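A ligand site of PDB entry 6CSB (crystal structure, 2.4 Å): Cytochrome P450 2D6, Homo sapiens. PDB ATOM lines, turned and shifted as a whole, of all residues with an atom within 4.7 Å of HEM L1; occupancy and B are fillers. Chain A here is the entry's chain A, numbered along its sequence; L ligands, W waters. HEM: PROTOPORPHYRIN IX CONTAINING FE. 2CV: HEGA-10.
FE of HEM L1 is bound by O44 of 2CV L2, 2.3 Å away.
O of Phe 414 lies within hydrogen-bond range of N of Cys 421, 3.1 Å away.
SG of Cys 421 lies close to N of Gly 423 (3.3 Å).
NH1 of Arg 419 lies within hydrogen-bond range of O of Phe 98 (3.2 Å).
O of Val 97 is in hydrogen-bond range of NH1 of Arg 419 (3.2 Å).
The guanidinium group of Arg 110 lies within hydrogen-bond range of the backbone carbonyl oxygen of Ala 420.
O of Ala 283 lies within hydrogen-bond range of OG1 of Thr 287, at 2.7 Å.
The backbone carbonyl oxygen of Gly 284 sits at hydrogen-bond distance from the side-chain hydroxyl of Thr 288, at 2.7 Å.
The side-chain hydroxyl of Thr 291 is in hydrogen-bond range of the backbone carbonyl oxygen of Thr 287 (2.8 Å).
FE of HEM L1 is bound by SG of Cys 421 (2.4 Å).
A ring nitrogen (NE2) of His 354 sits at hydrogen-bond distance from an oxygen (O2A) of HEM L1 (2.7 Å).
An oxygen (O1A) of HEM L1 lies within salt-bridge range of the guanidinium group (NH2) of Arg 79.
OG of Ser 415 is in hydrogen-bond range of O2A of HEM L1 (2.7 Å).
NH1 of Arg 419 lies within salt-bridge range of O2D of HEM L1.
The indole nitrogen (NE1) of Trp 106 lies within hydrogen-bond range of an oxygen (O1D) of HEM L1.
NH1 of Arg 110 lies within salt-bridge range of O1D of HEM L1.
O of Ala 283 sits close to O44 of 2CV L2.
Water W2 lies within hydrogen-bond range of an oxygen (O2A) of HEM L1 (2.8 Å), the backbone NH (N) of Val 352 (2.9 Å) and the side-chain hydroxyl (OG) of Ser 415 (3.4 Å).
Water W1 bridges the side-chain amide nitrogen (NE2) of Gln 342 and the side-chain hydroxyl (OG1) of Thr 291.
The backbone carbonyl oxygen (O) of Phe 98 sits close to an oxygen (O2D) of HEM L1 (3.4 Å).
The backbone carbonyl oxygen (O) of Ala 283 sits close to a nitrogen (NC) of HEM L1.
O of Val 97 touches O2D of HEM L1, at 3.7 Å.
CD2 of Leu 167 touches CBC of HEM L1, 3.99 Å away.
Leu 280 touches HEM L1 (CD2 to CAC, 3.9 Å).
CA of Gly 284 touches C2C of HEM L1, 3.4 Å away.
OG1 of Thr 287 touches C4B of HEM L1 (3.5 Å).
Thr 288 touches HEM L1.
OG1 of Thr 291 touches CBB of HEM L1, at 3.6 Å.
Gln 342 touches HEM L1 (NE2 to CBB, 3.7 Å).
CG2 of Val 352 touches CAA of HEM L1 (3.5 Å).
Leu 377 touches HEM L1.
Pro 413 touches HEM L1.
Phe 414 touches HEM L1.
CG of Leu 422 touches CMD of HEM L1, 3.6 Å away.
Gly 423 touches HEM L1.
Leu 426 touches HEM L1 (CD2 to CBC, 3.7 Å).
CB of Ala 427 touches CAB of HEM L1, 3.8 Å away.
Within 4 Å of HEM L1: Arg 79, Val 97, Phe 98, Trp 106, Arg 110, Leu 167, Leu 280, Ala 283, Gly 284, Thr 287, Thr 288, Thr 291, Gln 342, Val 352, His 354, Leu 377, Pro 413, Phe 414, Ser 415, Arg 419, Cys 421, Leu 422, Gly 423, Leu 426 and Ala 427.
The nearest printed residue that does not touch HEM L1 is Val 348 (4.003 Å).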
ATOM      1  N   LEU A  69      -8.292  13.802 -21.027  1.00  0.00           N
ATOM      2  CA  LEU A  69      -8.591  15.204 -20.732  1.00  0.00           C
ATOM      3  C   LEU A  69      -7.408  16.135 -20.946  1.00  0.00           C
ATOM      4  O   LEU A  69      -7.608  17.341 -21.094  1.00  0.00           O
ATOM      5  CB  LEU A  69      -9.084  15.354 -19.287  1.00  0.00           C
ATOM      6  CG  LEU A  69     -10.427  14.758 -18.892  1.00  0.00           C
ATOM      7  CD1 LEU A  69     -10.788  15.224 -17.499  1.00  0.00           C
ATOM      8  CD2 LEU A  69     -11.520  15.134 -19.906  1.00  0.00           C
ATOM      9  N   ARG A  79     -19.197  19.700 -24.069  1.00  0.00           N
ATOM     10  CA  ARG A  79     -20.257  19.204 -23.182  1.00  0.00           C
ATOM     11  C   ARG A  79     -21.324  18.495 -23.998  1.00  0.00           C
ATOM     12  O   ARG A  79     -21.637  18.941 -25.100  1.00  0.00           O
ATOM     13  CB  ARG A  79     -20.922  20.346 -22.386  1.00  0.00           C
ATOM     14  CG  ARG A  79     -20.047  21.026 -21.347  1.00  0.00           C
ATOM     15  CD  ARG A  79     -19.622  20.112 -20.227  1.00  0.00           C
ATOM     16  NE  ARG A  79     -18.995  20.879 -19.156  1.00  0.00           N
ATOM     17  CZ  ARG A  79     -18.035  20.417 -18.359  1.00  0.00           C
ATOM     18  NH1 ARG A  79     -17.527  21.220 -17.418  1.00  0.00           N
ATOM     19  NH2 ARG A  79     -17.580  19.159 -18.492  1.00  0.00           N
ATOM     20  N   VAL A  97     -21.172  29.208 -18.603  1.00  0.00           N
ATOM     21  CA  VAL A  97     -19.858  28.587 -18.631  1.00  0.00           C
ATOM     22  C   VAL A  97     -19.957  27.076 -18.422  1.00  0.00           C
ATOM     23  O   VAL A  97     -19.334  26.306 -19.138  1.00  0.00           O
ATOM     24  CB  VAL A  97     -18.916  29.213 -17.582  1.00  0.00           C
ATOM     25  CG1 VAL A  97     -17.528  28.626 -17.735  1.00  0.00           C
ATOM     26  CG2 VAL A  97     -18.895  30.687 -17.703  1.00  0.00           C
ATOM     27  N   PHE A  98     -20.733  26.655 -17.407  1.00  0.00           N
ATOM     28  CA  PHE A  98     -20.689  25.273 -16.930  1.00  0.00           C
ATOM     29  C   PHE A  98     -21.078  24.271 -18.025  1.00  0.00           C
ATOM     30  O   PHE A  98     -20.346  23.321 -18.316  1.00  0.00           O
ATOM     31  CB  PHE A  98     -21.620  25.141 -15.717  1.00  0.00           C
ATOM     32  CG  PHE A  98     -21.369  23.907 -14.880  1.00  0.00           C
ATOM     33  CD1 PHE A  98     -20.412  23.922 -13.883  1.00  0.00           C
ATOM     34  CD2 PHE A  98     -22.113  22.747 -15.080  1.00  0.00           C
ATOM     35  CE1 PHE A  98     -20.174  22.785 -13.098  1.00  0.00           C
ATOM     36  CE2 PHE A  98     -21.897  21.608 -14.296  1.00  0.00           C
ATOM     37  CZ  PHE A  98     -20.928  21.631 -13.307  1.00  0.00           C
ATOM     38  N   TRP A 106     -18.198  29.577 -24.838  1.00  0.00           N
ATOM     39  CA  TRP A 106     -17.606  29.024 -23.634  1.00  0.00           C
ATOM     40  C   TRP A 106     -16.312  29.743 -23.316  1.00  0.00           C
ATOM     41  O   TRP A 106     -16.061  30.128 -22.167  1.00  0.00           O
ATOM     42  CB  TRP A 106     -17.326  27.524 -23.763  1.00  0.00           C
ATOM     43  CG  TRP A 106     -16.398  27.044 -22.701  1.00  0.00           C
ATOM     44  CD1 TRP A 106     -16.717  26.753 -21.380  1.00  0.00           C
ATOM     45  CD2 TRP A 106     -14.975  26.831 -22.814  1.00  0.00           C
ATOM     46  NE1 TRP A 106     -15.581  26.375 -20.689  1.00  0.00           N
ATOM     47  CE2 TRP A 106     -14.504  26.415 -21.534  1.00  0.00           C
ATOM     48  CE3 TRP A 106     -14.070  26.947 -23.869  1.00  0.00           C
ATOM     49  CZ2 TRP A 106     -13.163  26.094 -21.297  1.00  0.00           C
ATOM     50  CZ3 TRP A 106     -12.719  26.661 -23.626  1.00  0.00           C
ATOM     51  CH2 TRP A 106     -12.283  26.234 -22.338  1.00  0.00           C
ATOM     52  N   ARG A 110     -15.291  31.700 -19.947  1.00  0.00           N
ATOM     53  CA  ARG A 110     -14.280  31.024 -19.132  1.00  0.00           C
ATOM     54  C   ARG A 110     -13.105  31.960 -18.836  1.00  0.00           C
ATOM     55  O   ARG A 110     -12.671  32.069 -17.692  1.00  0.00           O
ATOM     56  CB  ARG A 110     -13.810  29.753 -19.854  1.00  0.00           C
ATOM     57  CG  ARG A 110     -12.595  29.079 -19.247  1.00  0.00           C
ATOM     58  CD  ARG A 110     -12.966  28.077 -18.162  1.00  0.00           C
ATOM     59  NE  ARG A 110     -11.784  27.600 -17.460  1.00  0.00           N
ATOM     60  CZ  ARG A 110     -11.739  26.516 -16.685  1.00  0.00           C
ATOM     61  NH1 ARG A 110     -12.814  25.760 -16.514  1.00  0.00           N
ATOM     62  NH2 ARG A 110     -10.605  26.210 -16.056  1.00  0.00           N
ATOM     63  N   ILE A 164     -20.148  33.315  -2.501  1.00  0.00           N
ATOM     64  CA  ILE A 164     -20.585  33.485  -3.896  1.00  0.00           C
ATOM     65  C   ILE A 164     -21.276  34.842  -4.090  1.00  0.00           C
ATOM     66  O   ILE A 164     -20.963  35.585  -5.024  1.00  0.00           O
ATOM     67  CB  ILE A 164     -21.504  32.336  -4.358  1.00  0.00           C
ATOM     68  CG1 ILE A 164     -20.852  30.960  -4.119  1.00  0.00           C
ATOM     69  CG2 ILE A 164     -21.869  32.515  -5.858  1.00  0.00           C
ATOM     70  CD1 ILE A 164     -19.740  30.644  -5.113  1.00  0.00           C
ATOM     71  N   LEU A 167     -18.630  37.425  -4.262  1.00  0.00           N
ATOM     72  CA  LEU A 167     -17.954  37.365  -5.546  1.00  0.00           C
ATOM     73  C   LEU A 167     -18.801  37.989  -6.645  1.00  0.00           C
ATOM     74  O   LEU A 167     -18.309  38.784  -7.457  1.00  0.00           O
ATOM     75  CB  LEU A 167     -17.634  35.892  -5.890  1.00  0.00           C
ATOM     76  CG  LEU A 167     -17.421  35.574  -7.394  1.00  0.00           C
ATOM     77  CD1 LEU A 167     -16.153  36.219  -7.921  1.00  0.00           C
ATOM     78  CD2 LEU A 167     -17.405  34.081  -7.691  1.00  0.00           C
ATOM     79  N   LEU A 280     -22.242  29.965 -11.205  1.00  0.00           N
ATOM     80  CA  LEU A 280     -21.296  30.136 -10.111  1.00  0.00           C
ATOM     81  C   LEU A 280     -21.909  29.716  -8.772  1.00  0.00           C
ATOM     82  O   LEU A 280     -21.245  29.060  -7.962  1.00  0.00           O
ATOM     83  CB  LEU A 280     -20.804  31.591 -10.059  1.00  0.00           C
ATOM     84  CG  LEU A 280     -19.918  32.007 -11.250  1.00  0.00           C
ATOM     85  CD1 LEU A 280     -19.646  33.519 -11.249  1.00  0.00           C
ATOM     86  CD2 LEU A 280     -18.605  31.210 -11.315  1.00  0.00           C
ATOM     87  N   ALA A 283     -22.402  25.627  -9.085  1.00  0.00           N
ATOM     88  CA  ALA A 283     -21.173  24.855  -9.039  1.00  0.00           C
ATOM     89  C   ALA A 283     -20.383  25.085  -7.753  1.00  0.00           C
ATOM     90  O   ALA A 283     -19.610  24.206  -7.346  1.00  0.00           O
ATOM     91  CB  ALA A 283     -20.299  25.204 -10.261  1.00  0.00           C
ATOM     92  N   GLY A 284     -20.574  26.215  -7.075  1.00  0.00           N
ATOM     93  CA  GLY A 284     -19.661  26.545  -6.005  1.00  0.00           C
ATOM     94  C   GLY A 284     -20.235  26.463  -4.613  1.00  0.00           C
ATOM     95  O   GLY A 284     -19.484  26.565  -3.645  1.00  0.00           O
ATOM     96  N   THR A 287     -20.830  22.098  -3.423  1.00  0.00           N
ATOM     97  CA  THR A 287     -19.531  21.434  -3.420  1.00  0.00           C
ATOM     98  C   THR A 287     -18.701  21.863  -2.214  1.00  0.00           C
ATOM     99  O   THR A 287     -18.207  21.017  -1.463  1.00  0.00           O
ATOM    100  CB  THR A 287     -18.743  21.758  -4.685  1.00  0.00           C
ATOM    101  OG1 THR A 287     -18.872  23.159  -4.928  1.00  0.00           O
ATOM    102  CG2 THR A 287     -19.236  20.908  -5.890  1.00  0.00           C
ATOM    103  N   THR A 288     -18.564  23.183  -2.012  1.00  0.00           N
ATOM    104  CA  THR A 288     -17.681  23.679  -0.978  1.00  0.00           C
ATOM    105  C   THR A 288     -18.249  23.355   0.402  1.00  0.00           C
ATOM    106  O   THR A 288     -17.537  22.883   1.287  1.00  0.00           O
ATOM    107  CB  THR A 288     -17.475  25.184  -1.146  1.00  0.00           C
ATOM    108  OG1 THR A 288     -17.290  25.484  -2.549  1.00  0.00           O
ATOM    109  CG2 THR A 288     -16.259  25.659  -0.383  1.00  0.00           C
ATOM    110  N   THR A 291     -18.029  19.691   1.229  1.00  0.00           N
ATOM    111  CA  THR A 291     -16.657  19.367   1.617  1.00  0.00           C
ATOM    112  C   THR A 291     -16.404  19.751   3.068  1.00  0.00           C
ATOM    113  O   THR A 291     -15.822  18.964   3.839  1.00  0.00           O
ATOM    114  CB  THR A 291     -15.665  20.056   0.686  1.00  0.00           C
ATOM    115  OG1 THR A 291     -15.920  19.642  -0.672  1.00  0.00           O
ATOM    116  CG2 THR A 291     -14.233  19.669   1.010  1.00  0.00           C
ATOM    117  N   GLN A 342     -10.854  16.161   1.152  1.00  0.00           N
ATOM    118  CA  GLN A 342     -11.308  16.181  -0.238  1.00  0.00           C
ATOM    119  C   GLN A 342     -11.189  14.818  -0.917  1.00  0.00           C
ATOM    120  O   GLN A 342     -12.087  14.401  -1.660  1.00  0.00           O
ATOM    121  CB  GLN A 342     -10.484  17.203  -1.018  1.00  0.00           C
ATOM    122  CG  GLN A 342     -10.781  18.625  -0.644  1.00  0.00           C
ATOM    123  CD  GLN A 342     -10.405  19.574  -1.755  1.00  0.00           C
ATOM    124  OE1 GLN A 342      -9.301  20.096  -1.758  1.00  0.00           O
ATOM    125  NE2 GLN A 342     -11.316  19.773  -2.712  1.00  0.00           N
ATOM    126  N   ILE A 347     -16.446  14.024  -3.188  1.00  0.00           N
ATOM    127  CA  ILE A 347     -17.814  14.518  -3.306  1.00  0.00           C
ATOM    128  C   ILE A 347     -18.340  14.597  -4.746  1.00  0.00           C
ATOM    129  O   ILE A 347     -19.551  14.778  -4.933  1.00  0.00           O
ATOM    130  CB  ILE A 347     -17.962  15.911  -2.655  1.00  0.00           C
ATOM    131  CG1 ILE A 347     -17.271  16.967  -3.510  1.00  0.00           C
ATOM    132  CG2 ILE A 347     -17.434  15.907  -1.214  1.00  0.00           C
ATOM    133  CD1 ILE A 347     -17.836  18.338  -3.311  1.00  0.00           C
ATOM    134  N   VAL A 348     -17.470  14.512  -5.754  1.00  0.00           N
ATOM    135  CA  VAL A 348     -17.900  14.474  -7.159  1.00  0.00           C
ATOM    136  C   VAL A 348     -17.338  13.212  -7.794  1.00  0.00           C
ATOM    137  O   VAL A 348     -16.376  13.266  -8.577  1.00  0.00           O
ATOM    138  CB  VAL A 348     -17.468  15.741  -7.935  1.00  0.00           C
ATOM    139  CG1 VAL A 348     -18.354  15.939  -9.179  1.00  0.00           C
ATOM    140  CG2 VAL A 348     -17.554  16.978  -7.063  1.00  0.00           C
ATOM    141  N   GLY A 351     -17.481  13.001 -11.648  1.00  0.00           N
ATOM    142  CA  GLY A 351     -17.166  14.262 -12.273  1.00  0.00           C
ATOM    143  C   GLY A 351     -18.376  14.884 -12.932  1.00  0.00           C
ATOM    144  O   GLY A 351     -19.515  14.736 -12.485  1.00  0.00           O
ATOM    145  N   VAL A 352     -18.098  15.591 -14.031  1.00  0.00           N
ATOM    146  CA  VAL A 352     -19.100  16.221 -14.885  1.00  0.00           C
ATOM    147  C   VAL A 352     -18.843  15.724 -16.304  1.00  0.00           C
ATOM    148  O   VAL A 352     -17.697  15.706 -16.763  1.00  0.00           O
ATOM    149  CB  VAL A 352     -19.034  17.764 -14.810  1.00  0.00           C
ATOM    150  CG1 VAL A 352     -20.013  18.444 -15.788  1.00  0.00           C
ATOM    151  CG2 VAL A 352     -19.247  18.232 -13.393  1.00  0.00           C
ATOM    152  N   HIS A 354     -18.250  15.056 -20.179  1.00  0.00           N
ATOM    153  CA  HIS A 354     -17.665  15.655 -21.352  1.00  0.00           C
ATOM    154  C   HIS A 354     -18.247  14.986 -22.598  1.00  0.00           C
ATOM    155  O   HIS A 354     -18.965  13.989 -22.524  1.00  0.00           O
ATOM    156  CB  HIS A 354     -16.148  15.483 -21.328  1.00  0.00           C
ATOM    157  CG  HIS A 354     -15.470  16.230 -20.209  1.00  0.00           C
ATOM    158  ND1 HIS A 354     -14.393  17.064 -20.429  1.00  0.00           N
ATOM    159  CD2 HIS A 354     -15.696  16.234 -18.873  1.00  0.00           C
ATOM    160  CE1 HIS A 354     -13.982  17.554 -19.270  1.00  0.00           C
ATOM    161  NE2 HIS A 354     -14.747  17.069 -18.312  1.00  0.00           N
ATOM    162  N   LEU A 377     -13.605  10.196 -11.260  1.00  0.00           N
ATOM    163  CA  LEU A 377     -12.630  10.816 -10.372  1.00  0.00           C
ATOM    164  C   LEU A 377     -12.414   9.967  -9.118  1.00  0.00           C
ATOM    165  O   LEU A 377     -11.290   9.870  -8.613  1.00  0.00           O
ATOM    166  CB  LEU A 377     -13.085  12.241 -10.006  1.00  0.00           C
ATOM    167  CG  LEU A 377     -13.403  13.172 -11.190  1.00  0.00           C
ATOM    168  CD1 LEU A 377     -13.881  14.548 -10.724  1.00  0.00           C
ATOM    169  CD2 LEU A 377     -12.191  13.347 -12.109  1.00  0.00           C
ATOM    170  N   PRO A 413      -9.605  16.154  -7.405  1.00  0.00           N
ATOM    171  CA  PRO A 413     -11.021  16.377  -7.075  1.00  0.00           C
ATOM    172  C   PRO A 413     -11.648  17.446  -7.942  1.00  0.00           C
ATOM    173  O   PRO A 413     -12.866  17.586  -7.926  1.00  0.00           O
ATOM    174  CB  PRO A 413     -10.976  16.814  -5.605  1.00  0.00           C
ATOM    175  CG  PRO A 413      -9.674  17.555  -5.506  1.00  0.00           C
ATOM    176  CD  PRO A 413      -8.713  16.747  -6.375  1.00  0.00           C
ATOM    177  N   PHE A 414     -10.842  18.191  -8.711  1.00  0.00           N
ATOM    178  CA  PHE A 414     -11.328  19.251  -9.578  1.00  0.00           C
ATOM    179  C   PHE A 414     -11.259  18.883 -11.064  1.00  0.00           C
ATOM    180  O   PHE A 414     -11.396  19.769 -11.910  1.00  0.00           O
ATOM    181  CB  PHE A 414     -10.539  20.548  -9.313  1.00  0.00           C
ATOM    182  CG  PHE A 414     -10.664  21.075  -7.876  1.00  0.00           C
ATOM    183  CD1 PHE A 414      -9.619  20.924  -6.965  1.00  0.00           C
ATOM    184  CD2 PHE A 414     -11.807  21.766  -7.460  1.00  0.00           C
ATOM    185  CE1 PHE A 414      -9.710  21.444  -5.664  1.00  0.00           C
ATOM    186  CE2 PHE A 414     -11.923  22.301  -6.142  1.00  0.00           C
ATOM    187  CZ  PHE A 414     -10.871  22.121  -5.252  1.00  0.00           C
ATOM    188  N   SER A 415     -11.030  17.606 -11.382  1.00  0.00           N
ATOM    189  CA  SER A 415     -10.815  17.118 -12.743  1.00  0.00           C
ATOM    190  C   SER A 415      -9.511  17.664 -13.312  1.00  0.00           C
ATOM    191  O   SER A 415      -8.589  17.970 -12.554  1.00  0.00           O
ATOM    192  CB  SER A 415     -12.013  17.455 -13.637  1.00  0.00           C
ATOM    193  OG  SER A 415     -11.962  16.692 -14.832  1.00  0.00           O
ATOM    194  N   ARG A 419     -11.429  22.175 -18.999  1.00  0.00           N
ATOM    195  CA  ARG A 419     -12.698  22.331 -18.320  1.00  0.00           C
ATOM    196  C   ARG A 419     -12.592  22.139 -16.821  1.00  0.00           C
ATOM    197  O   ARG A 419     -13.604  22.233 -16.116  1.00  0.00           O
ATOM    198  CB  ARG A 419     -13.695  21.343 -18.905  1.00  0.00           C
ATOM    199  CG  ARG A 419     -14.190  21.745 -20.243  1.00  0.00           C
ATOM    200  CD  ARG A 419     -15.199  22.877 -20.053  1.00  0.00           C
ATOM    201  NE  ARG A 419     -15.930  23.004 -21.267  1.00  0.00           N
ATOM    202  CZ  ARG A 419     -17.179  23.385 -21.398  1.00  0.00           C
ATOM    203  NH1 ARG A 419     -17.920  23.766 -20.355  1.00  0.00           N
ATOM    204  NH2 ARG A 419     -17.694  23.377 -22.622  1.00  0.00           N
ATOM    205  N   ALA A 420     -11.404  21.837 -16.306  1.00  0.00           N
ATOM    206  CA  ALA A 420     -11.229  21.636 -14.872  1.00  0.00           C
ATOM    207  C   ALA A 420     -11.753  22.856 -14.104  1.00  0.00           C
ATOM    208  O   ALA A 420     -11.701  23.987 -14.586  1.00  0.00           O
ATOM    209  CB  ALA A 420      -9.751  21.381 -14.554  1.00  0.00           C
ATOM    210  N   CYS A 421     -12.315  22.582 -12.930  1.00  0.00           N
ATOM    211  CA  CYS A 421     -13.010  23.574 -12.126  1.00  0.00           C
ATOM    212  C   CYS A 421     -12.324  24.939 -12.160  1.00  0.00           C
ATOM    213  O   CYS A 421     -11.152  25.066 -11.811  1.00  0.00           O
ATOM    214  CB  CYS A 421     -13.063  23.073 -10.688  1.00  0.00           C
ATOM    215  SG  CYS A 421     -13.785  24.227  -9.544  1.00  0.00           S
ATOM    216  N   LEU A 422     -13.053  25.969 -12.605  1.00  0.00           N
ATOM    217  CA  LEU A 422     -12.472  27.308 -12.596  1.00  0.00           C
ATOM    218  C   LEU A 422     -12.498  27.924 -11.203  1.00  0.00           C
ATOM    219  O   LEU A 422     -11.757  28.888 -10.952  1.00  0.00           O
ATOM    220  CB  LEU A 422     -13.180  28.251 -13.600  1.00  0.00           C
ATOM    221  CG  LEU A 422     -14.673  28.577 -13.457  1.00  0.00           C
ATOM    222  CD1 LEU A 422     -15.042  29.616 -12.334  1.00  0.00           C
ATOM    223  CD2 LEU A 422     -15.213  29.078 -14.807  1.00  0.00           C
ATOM    224  N   GLY A 423     -13.307  27.395 -10.292  1.00  0.00           N
ATOM    225  CA  GLY A 423     -13.375  27.940  -8.961  1.00  0.00           C
ATOM    226  C   GLY A 423     -12.333  27.398  -8.004  1.00  0.00           C
ATOM    227  O   GLY A 423     -12.298  27.833  -6.866  1.00  0.00           O
ATOM    228  N   LEU A 426     -10.591  29.768  -5.463  1.00  0.00           N
ATOM    229  CA  LEU A 426     -11.512  30.253  -4.439  1.00  0.00           C
ATOM    230  C   LEU A 426     -11.898  29.139  -3.446  1.00  0.00           C
ATOM    231  O   LEU A 426     -12.003  29.383  -2.241  1.00  0.00           O
ATOM    232  CB  LEU A 426     -12.757  30.863  -5.090  1.00  0.00           C
ATOM    233  CG  LEU A 426     -13.858  31.448  -4.156  1.00  0.00           C
ATOM    234  CD1 LEU A 426     -13.339  32.458  -3.097  1.00  0.00           C
ATOM    235  CD2 LEU A 426     -14.949  32.110  -4.988  1.00  0.00           C
ATOM    236  N   ALA A 427     -12.122  27.910  -3.947  1.00  0.00           N
ATOM    237  CA  ALA A 427     -12.444  26.801  -3.040  1.00  0.00           C
ATOM    238  C   ALA A 427     -11.277  26.499  -2.103  1.00  0.00           C
ATOM    239  O   ALA A 427     -11.495  26.241  -0.915  1.00  0.00           O
ATOM    240  CB  ALA A 427     -12.838  25.538  -3.809  1.00  0.00           C
ATOM    241  N   GLU A 430     -11.444  29.053   0.483  1.00  0.00           N
ATOM    242  CA  GLU A 430     -12.564  28.851   1.393  1.00  0.00           C
ATOM    243  C   GLU A 430     -12.314  27.672   2.344  1.00  0.00           C
ATOM    244  O   GLU A 430     -12.571  27.771   3.546  1.00  0.00           O
ATOM    245  CB  GLU A 430     -13.844  28.634   0.590  1.00  0.00           C
ATOM    246  CG  GLU A 430     -14.532  29.886   0.071  1.00  0.00           C
ATOM    247  CD  GLU A 430     -15.893  29.571  -0.579  1.00  0.00           C
ATOM    248  OE1 GLU A 430     -16.909  29.564   0.146  1.00  0.00           O
ATOM    249  OE2 GLU A 430     -15.946  29.279  -1.812  1.00  0.00           O
ATOM    250  N   LEU A 431     -11.833  26.543   1.821  1.00  0.00           N
ATOM    251  CA  LEU A 431     -11.642  25.384   2.670  1.00  0.00           C
ATOM    252  C   LEU A 431     -10.618  25.671   3.771  1.00  0.00           C
ATOM    253  O   LEU A 431     -10.845  25.361   4.936  1.00  0.00           O
ATOM    254  CB  LEU A 431     -11.192  24.183   1.830  1.00  0.00           C
ATOM    255  CG  LEU A 431     -12.185  23.657   0.803  1.00  0.00           C
ATOM    256  CD1 LEU A 431     -11.620  22.429   0.002  1.00  0.00           C
ATOM    257  CD2 LEU A 431     -13.530  23.346   1.486  1.00  0.00           C
HETATM  258  CHA HEM L   1     -16.350  22.609 -12.696  1.00  0.00           C
HETATM  259  CHB HEM L   1     -15.416  20.411  -8.525  1.00  0.00           C
HETATM  260  CHC HEM L   1     -15.908  24.625  -6.190  1.00  0.00           C
HETATM  261  CHD HEM L   1     -17.285  26.762 -10.357  1.00  0.00           C
HETATM  262  C1A HEM L   1     -16.059  21.618 -11.797  1.00  0.00           C
HETATM  263  C2A HEM L   1     -15.848  20.198 -12.065  1.00  0.00           C
HETATM  264  C3A HEM L   1     -15.588  19.597 -10.905  1.00  0.00           C
HETATM  265  C4A HEM L   1     -15.628  20.624  -9.864  1.00  0.00           C
HETATM  266  CMA HEM L   1     -15.319  18.093 -10.654  1.00  0.00           C
HETATM  267  CAA HEM L   1     -15.937  19.462 -13.435  1.00  0.00           C
HETATM  268  CBA HEM L   1     -14.757  19.735 -14.370  1.00  0.00           C
HETATM  269  CGA HEM L   1     -14.911  18.928 -15.659  1.00  0.00           C
HETATM  270  O1A HEM L   1     -15.741  19.307 -16.533  1.00  0.00           O
HETATM  271  O2A HEM L   1     -14.183  17.905 -15.831  1.00  0.00           O
HETATM  272  C1B HEM L   1     -15.465  21.353  -7.533  1.00  0.00           C
HETATM  273  C2B HEM L   1     -15.167  21.090  -6.151  1.00  0.00           C
HETATM  274  C3B HEM L   1     -15.302  22.251  -5.488  1.00  0.00           C
HETATM  275  C4B HEM L   1     -15.677  23.276  -6.446  1.00  0.00           C
HETATM  276  CMB HEM L   1     -14.771  19.682  -5.629  1.00  0.00           C
HETATM  277  CAB HEM L   1     -15.115  22.514  -3.973  1.00  0.00           C
HETATM  278  CBB HEM L   1     -14.433  21.709  -3.162  1.00  0.00           C
HETATM  279  C1C HEM L   1     -16.281  25.587  -7.115  1.00  0.00           C
HETATM  280  C2C HEM L   1     -16.421  27.022  -6.883  1.00  0.00           C
HETATM  281  C3C HEM L   1     -16.824  27.616  -8.027  1.00  0.00           C
HETATM  282  C4C HEM L   1     -16.917  26.566  -9.041  1.00  0.00           C
HETATM  283  CMC HEM L   1     -16.182  27.691  -5.499  1.00  0.00           C
HETATM  284  CAC HEM L   1     -17.146  29.115  -8.331  1.00  0.00           C
HETATM  285  CBC HEM L   1     -16.667  30.156  -7.656  1.00  0.00           C
HETATM  286  C1D HEM L   1     -17.169  25.828 -11.373  1.00  0.00           C
HETATM  287  C2D HEM L   1     -17.491  26.015 -12.779  1.00  0.00           C
HETATM  288  C3D HEM L   1     -17.229  24.843 -13.414  1.00  0.00           C
HETATM  289  C4D HEM L   1     -16.737  23.901 -12.439  1.00  0.00           C
HETATM  290  CMD HEM L   1     -18.046  27.354 -13.382  1.00  0.00           C
HETATM  291  CAD HEM L   1     -17.359  24.500 -14.928  1.00  0.00           C
HETATM  292  CBD HEM L   1     -16.044  24.851 -15.642  1.00  0.00           C
HETATM  293  CGD HEM L   1     -16.162  24.703 -17.154  1.00  0.00           C
HETATM  294  O1D HEM L   1     -15.433  25.405 -17.905  1.00  0.00           O
HETATM  295  O2D HEM L   1     -17.025  23.909 -17.631  1.00  0.00           O
HETATM  296  NA  HEM L   1     -15.906  21.827 -10.441  1.00  0.00           N
HETATM  297  NB  HEM L   1     -15.775  22.675  -7.687  1.00  0.00           N
HETATM  298  NC  HEM L   1     -16.581  25.365  -8.443  1.00  0.00           N
HETATM  299  ND  HEM L   1     -16.721  24.523 -11.205  1.00  0.00           N
HETATM  300 FE   HEM L   1     -16.060  23.634  -9.499  1.00  0.00          FE
HETATM  301  N33 2CV L   2     -21.960  15.565  -9.993  1.00  0.00           N
HETATM  302  C36 2CV L   2     -22.496  16.796 -10.549  1.00  0.00           C
HETATM  303  C37 2CV L   2     -21.332  17.779 -10.684  1.00  0.00           C
HETATM  304  C40 2CV L   2     -21.114  18.631  -9.434  1.00  0.00           C
HETATM  305  C41 2CV L   2     -20.878  20.122  -9.700  1.00  0.00           C
HETATM  306  C42 2CV L   2     -19.421  20.561  -9.531  1.00  0.00           C
HETATM  307  C43 2CV L   2     -19.281  22.027  -9.893  1.00  0.00           C
HETATM  308  O44 2CV L   2     -18.184  22.664  -9.240  1.00  0.00           O
HETATM  309  O51 2CV L   2     -21.666  20.907  -8.796  1.00  0.00           O
HETATM  310  O53 2CV L   2     -18.562  19.829 -10.399  1.00  0.00           O
HETATM  311  O   HOH W   1     -13.638  18.425  -2.297  1.00  0.00           O
HETATM  312  O   HOH W   2     -15.251  15.818 -14.380  1.00  0.00           O
